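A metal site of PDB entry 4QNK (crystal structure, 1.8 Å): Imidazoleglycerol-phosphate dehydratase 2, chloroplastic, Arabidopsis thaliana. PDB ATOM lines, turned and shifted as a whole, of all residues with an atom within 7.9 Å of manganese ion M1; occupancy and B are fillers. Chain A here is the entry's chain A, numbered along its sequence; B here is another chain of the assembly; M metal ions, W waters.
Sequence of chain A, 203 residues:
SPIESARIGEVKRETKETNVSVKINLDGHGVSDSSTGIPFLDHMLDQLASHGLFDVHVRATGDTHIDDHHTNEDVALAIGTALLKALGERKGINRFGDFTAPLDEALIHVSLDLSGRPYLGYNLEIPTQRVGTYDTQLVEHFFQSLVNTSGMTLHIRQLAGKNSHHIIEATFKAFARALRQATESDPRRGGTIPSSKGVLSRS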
ATOM      1  N   PHE A  40      -6.244  -6.282 -10.187  1.00  0.00           N
ATOM      2  CA  PHE A  40      -7.137  -7.449 -10.292  1.00  0.00           C
ATOM      3  C   PHE A  40      -7.764  -7.740  -8.929  1.00  0.00           C
ATOM      4  O   PHE A  40      -8.915  -8.166  -8.812  1.00  0.00           O
ATOM      5  CB  PHE A  40      -6.446  -8.682 -10.897  1.00  0.00           C
ATOM      6  CG  PHE A  40      -7.416  -9.810 -11.183  1.00  0.00           C
ATOM      7  CD1 PHE A  40      -8.155  -9.837 -12.372  1.00  0.00           C
ATOM      8  CD2 PHE A  40      -7.604 -10.806 -10.242  1.00  0.00           C
ATOM      9  CE1 PHE A  40      -9.087 -10.860 -12.600  1.00  0.00           C
ATOM     10  CE2 PHE A  40      -8.492 -11.855 -10.488  1.00  0.00           C
ATOM     11  CZ  PHE A  40      -9.238 -11.870 -11.647  1.00  0.00           C
ATOM     12  N   HIS A  43     -10.622  -5.494  -8.252  1.00  0.00           N
ATOM     13  CA  HIS A  43     -11.779  -6.018  -9.029  1.00  0.00           C
ATOM     14  C   HIS A  43     -12.479  -7.162  -8.264  1.00  0.00           C
ATOM     15  O   HIS A  43     -13.730  -7.213  -8.183  1.00  0.00           O
ATOM     16  CB  HIS A  43     -11.301  -6.454 -10.444  1.00  0.00           C
ATOM     17  CG  HIS A  43     -12.376  -7.020 -11.299  1.00  0.00           C
ATOM     18  ND1 HIS A  43     -13.624  -6.449 -11.424  1.00  0.00           N
ATOM     19  CD2 HIS A  43     -12.377  -8.096 -12.126  1.00  0.00           C
ATOM     20  CE1 HIS A  43     -14.366  -7.188 -12.235  1.00  0.00           C
ATOM     21  NE2 HIS A  43     -13.605  -8.156 -12.717  1.00  0.00           N
ATOM     22  N   MET A  44     -11.691  -8.054  -7.655  1.00  0.00           N
ATOM     23  CA  MET A  44     -12.246  -9.135  -6.819  1.00  0.00           C
ATOM     24  C   MET A  44     -12.898  -8.607  -5.523  1.00  0.00           C
ATOM     25  O   MET A  44     -13.967  -9.091  -5.076  1.00  0.00           O
ATOM     26  CB  MET A  44     -11.180 -10.216  -6.547  1.00  0.00           C
ATOM     27  CG  MET A  44     -10.764 -10.996  -7.797  1.00  0.00           C
ATOM     28  SD  MET A  44     -12.125 -11.758  -8.728  1.00  0.00           S
ATOM     29  CE  MET A  44     -12.492 -10.604 -10.029  1.00  0.00           C
ATOM     30  N   GLN A  47     -16.190  -7.357  -6.368  1.00  0.00           N
ATOM     31  CA  GLN A  47     -17.124  -8.508  -6.434  1.00  0.00           C
ATOM     32  C   GLN A  47     -17.615  -8.947  -5.024  1.00  0.00           C
ATOM     33  O   GLN A  47     -18.794  -9.259  -4.837  1.00  0.00           O
ATOM     34  CB  GLN A  47     -16.483  -9.676  -7.192  1.00  0.00           C
ATOM     35  CG  GLN A  47     -16.273  -9.393  -8.678  1.00  0.00           C
ATOM     36  CD  GLN A  47     -17.538  -9.541  -9.463  1.00  0.00           C
ATOM     37  OE1 GLN A  47     -18.192 -10.565  -9.358  1.00  0.00           O
ATOM     38  NE2 GLN A  47     -17.900  -8.544 -10.254  1.00  0.00           N
ATOM     39  N   LEU A 103     -19.975 -18.711 -13.483  1.00  0.00           N
ATOM     40  CA  LEU A 103     -19.679 -17.587 -14.346  1.00  0.00           C
ATOM     41  C   LEU A 103     -19.383 -18.232 -15.700  1.00  0.00           C
ATOM     42  O   LEU A 103     -18.297 -18.826 -15.884  1.00  0.00           O
ATOM     43  CB  LEU A 103     -18.513 -16.744 -13.852  1.00  0.00           C
ATOM     44  CG  LEU A 103     -18.399 -15.343 -14.521  1.00  0.00           C
ATOM     45  CD1 LEU A 103     -17.192 -14.545 -14.075  1.00  0.00           C
ATOM     46  CD2 LEU A 103     -18.446 -15.300 -16.019  1.00  0.00           C
ATOM     47  N   HIS A 165      -9.818 -15.953 -15.460  1.00  0.00           N
ATOM     48  CA  HIS A 165     -10.601 -14.820 -14.941  1.00  0.00           C
ATOM     49  C   HIS A 165     -11.968 -15.307 -14.446  1.00  0.00           C
ATOM     50  O   HIS A 165     -12.398 -14.980 -13.304  1.00  0.00           O
ATOM     51  CB  HIS A 165     -10.681 -13.711 -16.029  1.00  0.00           C
ATOM     52  CG  HIS A 165     -11.285 -12.410 -15.579  1.00  0.00           C
ATOM     53  ND1 HIS A 165     -10.741 -11.192 -15.934  1.00  0.00           N
ATOM     54  CD2 HIS A 165     -12.420 -12.118 -14.906  1.00  0.00           C
ATOM     55  CE1 HIS A 165     -11.482 -10.216 -15.447  1.00  0.00           C
ATOM     56  NE2 HIS A 165     -12.537 -10.751 -14.858  1.00  0.00           N
ATOM     57  N   HIS A 166     -12.634 -16.156 -15.240  1.00  0.00           N
ATOM     58  CA  HIS A 166     -13.915 -16.735 -14.861  1.00  0.00           C
ATOM     59  C   HIS A 166     -13.839 -17.591 -13.588  1.00  0.00           C
ATOM     60  O   HIS A 166     -14.700 -17.483 -12.710  1.00  0.00           O
ATOM     61  CB  HIS A 166     -14.571 -17.569 -15.998  1.00  0.00           C
ATOM     62  CG  HIS A 166     -15.050 -16.742 -17.170  1.00  0.00           C
ATOM     63  ND1 HIS A 166     -15.606 -17.296 -18.311  1.00  0.00           N
ATOM     64  CD2 HIS A 166     -15.056 -15.422 -17.369  1.00  0.00           C
ATOM     65  CE1 HIS A 166     -15.915 -16.346 -19.157  1.00  0.00           C
ATOM     66  NE2 HIS A 166     -15.628 -15.188 -18.583  1.00  0.00           N
ATOM     67  N   GLU A 169     -13.138 -15.173 -10.550  1.00  0.00           N
ATOM     68  CA  GLU A 169     -14.314 -14.325 -10.311  1.00  0.00           C
ATOM     69  C   GLU A 169     -15.508 -15.116  -9.750  1.00  0.00           C
ATOM     70  O   GLU A 169     -16.175 -14.679  -8.789  1.00  0.00           O
ATOM     71  CB  GLU A 169     -14.693 -13.542 -11.555  1.00  0.00           C
ATOM     72  CG  GLU A 169     -15.778 -12.494 -11.289  1.00  0.00           C
ATOM     73  CD  GLU A 169     -15.955 -11.533 -12.430  1.00  0.00           C
ATOM     74  OE1 GLU A 169     -14.938 -11.094 -13.005  1.00  0.00           O
ATOM     75  OE2 GLU A 169     -17.107 -11.208 -12.765  1.00  0.00           O
ATOM     76  N   LYS A 173     -17.599 -14.606  -6.270  1.00  0.00           N
ATOM     77  CA  LYS A 173     -19.057 -14.530  -6.183  1.00  0.00           C
ATOM     78  C   LYS A 173     -19.645 -15.504  -5.163  1.00  0.00           C
ATOM     79  O   LYS A 173     -20.499 -15.126  -4.337  1.00  0.00           O
ATOM     80  CB  LYS A 173     -19.738 -14.737  -7.533  1.00  0.00           C
ATOM     81  CG  LYS A 173     -19.430 -13.687  -8.608  1.00  0.00           C
ATOM     82  CD  LYS A 173     -20.156 -14.090  -9.890  1.00  0.00           C
ATOM     83  CE  LYS A 173     -19.649 -13.510 -11.155  1.00  0.00           C
ATOM     84  NZ  LYS A 173     -19.495 -12.048 -11.199  1.00  0.00           N
ATOM     85  N   GLU B  17     -17.692  -1.131 -17.250  1.00  0.00           N
ATOM     86  CA  GLU B  17     -16.304  -1.513 -17.510  1.00  0.00           C
ATOM     87  C   GLU B  17     -15.756  -1.070 -18.862  1.00  0.00           C
ATOM     88  O   GLU B  17     -14.544  -0.934 -19.021  1.00  0.00           O
ATOM     89  CB  GLU B  17     -16.122  -3.037 -17.385  1.00  0.00           C
ATOM     90  CG  GLU B  17     -16.349  -3.580 -15.987  1.00  0.00           C
ATOM     91  CD  GLU B  17     -17.605  -4.407 -15.861  1.00  0.00           C
ATOM     92  OE1 GLU B  17     -18.689  -3.970 -16.306  1.00  0.00           O
ATOM     93  OE2 GLU B  17     -17.499  -5.524 -15.318  1.00  0.00           O
ATOM     94  N   ASP B  63     -11.251  -1.082 -18.979  1.00  0.00           N
ATOM     95  CA  ASP B  63     -10.375  -1.315 -17.832  1.00  0.00           C
ATOM     96  C   ASP B  63      -9.227  -2.280 -18.094  1.00  0.00           C
ATOM     97  O   ASP B  63      -9.071  -3.252 -17.376  1.00  0.00           O
ATOM     98  CB  ASP B  63     -11.207  -1.803 -16.635  1.00  0.00           C
ATOM     99  CG  ASP B  63     -12.090  -3.014 -16.966  1.00  0.00           C
ATOM    100  OD1 ASP B  63     -11.855  -3.728 -17.969  1.00  0.00           O
ATOM    101  OD2 ASP B  63     -13.028  -3.250 -16.188  1.00  0.00           O
ATOM    102  N   ILE B  66      -6.913  -3.923 -15.359  1.00  0.00           N
ATOM    103  CA  ILE B  66      -7.385  -5.157 -14.690  1.00  0.00           C
ATOM    104  C   ILE B  66      -6.945  -6.380 -15.505  1.00  0.00           C
ATOM    105  O   ILE B  66      -6.336  -7.310 -14.979  1.00  0.00           O
ATOM    106  CB  ILE B  66      -8.927  -5.181 -14.540  1.00  0.00           C
ATOM    107  CG1 ILE B  66      -9.407  -4.083 -13.574  1.00  0.00           C
ATOM    108  CG2 ILE B  66      -9.385  -6.550 -14.079  1.00  0.00           C
ATOM    109  CD1 ILE B  66     -10.917  -4.009 -13.388  1.00  0.00           C
ATOM    110  N   ASP B  67      -7.329  -6.383 -16.777  1.00  0.00           N
ATOM    111  CA  ASP B  67      -6.792  -7.237 -17.831  1.00  0.00           C
ATOM    112  C   ASP B  67      -7.570  -6.897 -19.121  1.00  0.00           C
ATOM    113  O   ASP B  67      -8.444  -6.029 -19.107  1.00  0.00           O
ATOM    114  CB  ASP B  67      -6.753  -8.761 -17.477  1.00  0.00           C
ATOM    115  CG  ASP B  67      -8.101  -9.415 -17.428  1.00  0.00           C
ATOM    116  OD1 ASP B  67      -8.145 -10.699 -17.360  1.00  0.00           O
ATOM    117  OD2 ASP B  67      -9.079  -8.655 -17.429  1.00  0.00           O
ATOM    118  N   HIS B  69      -9.723  -8.762 -20.601  1.00  0.00           N
ATOM    119  CA  HIS B  69     -10.893  -9.632 -20.677  1.00  0.00           C
ATOM    120  C   HIS B  69     -12.191  -8.843 -20.962  1.00  0.00           C
ATOM    121  O   HIS B  69     -12.955  -9.207 -21.860  1.00  0.00           O
ATOM    122  CB  HIS B  69     -11.047 -10.447 -19.390  1.00  0.00           C
ATOM    123  CG  HIS B  69     -12.132 -11.478 -19.391  1.00  0.00           C
ATOM    124  ND1 HIS B  69     -11.864 -12.822 -19.270  1.00  0.00           N
ATOM    125  CD2 HIS B  69     -13.487 -11.366 -19.422  1.00  0.00           C
ATOM    126  CE1 HIS B  69     -13.004 -13.493 -19.221  1.00  0.00           C
ATOM    127  NE2 HIS B  69     -13.989 -12.632 -19.365  1.00  0.00           N
ATOM    128  N   HIS B  70     -12.463  -7.793 -20.183  1.00  0.00           N
ATOM    129  CA  HIS B  70     -13.791  -7.121 -20.315  1.00  0.00           C
ATOM    130  C   HIS B  70     -13.903  -6.443 -21.685  1.00  0.00           C
ATOM    131  O   HIS B  70     -14.929  -6.540 -22.370  1.00  0.00           O
ATOM    132  CB  HIS B  70     -14.072  -6.127 -19.182  1.00  0.00           C
ATOM    133  CG  HIS B  70     -14.028  -6.736 -17.804  1.00  0.00           C
ATOM    134  ND1 HIS B  70     -13.733  -6.007 -16.665  1.00  0.00           N
ATOM    135  CD2 HIS B  70     -14.212  -7.999 -17.403  1.00  0.00           C
ATOM    136  CE1 HIS B  70     -13.729  -6.825 -15.624  1.00  0.00           C
ATOM    137  NE2 HIS B  70     -14.082  -8.034 -16.037  1.00  0.00           N
ATOM    138  N   GLU B  73     -14.311  -9.078 -24.564  1.00  0.00           N
ATOM    139  CA  GLU B  73     -15.672  -9.610 -24.525  1.00  0.00           C
ATOM    140  C   GLU B  73     -16.686  -8.598 -25.070  1.00  0.00           C
ATOM    141  O   GLU B  73     -17.516  -8.923 -25.906  1.00  0.00           O
ATOM    142  CB  GLU B  73     -16.051 -10.002 -23.084  1.00  0.00           C
ATOM    143  CG  GLU B  73     -17.430 -10.541 -22.956  1.00  0.00           C
ATOM    144  CD  GLU B  73     -17.685 -11.273 -21.650  1.00  0.00           C
ATOM    145  OE1 GLU B  73     -16.704 -11.441 -20.820  1.00  0.00           O
ATOM    146  OE2 GLU B  73     -18.867 -11.725 -21.509  1.00  0.00           O
HETATM  147 MN    MN M   1     -14.346  -9.528 -14.386  1.00  0.00          MN
HETATM  148 MN    MN M   2     -16.114 -13.250 -19.621  1.00  0.00          MN
HETATM  149  O   HOH W   1     -16.462  -8.741 -14.057  1.00  0.00           O
HETATM  150  O   HOH W   2     -15.654 -10.503 -15.824  1.00  0.00           O
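Manganese ion M1 is bound by the side-chain carboxylate (OE1) of Glu 169 (2.2 Å). Manganese ion M1 is bound by water W2, 2.2 Å away. Manganese ion M1 is bound by a ring nitrogen (NE2) of His 165 (2.2 Å). NE2 of His 70 of chain B is bound to manganese ion M1, 2.2 Å away. Manganese ion M1 is bound by water W1 (2.3 Å). NE2 of His 43 binds manganese ion M1 (2.3 Å).
The side-chain amino group of Lys 173 lies within salt-bridge range of the side-chain carboxylate of Glu 169 (3.0 Å). A ring nitrogen (ND1) of His 165 sits at hydrogen-bond distance from the side-chain carboxylate (OD1) of Asp 67 of chain B, at 3.0 Å. OD2 of Asp 63 of chain B sits at hydrogen-bond distance from ND1 of His 70 of chain B, at 2.9 Å.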
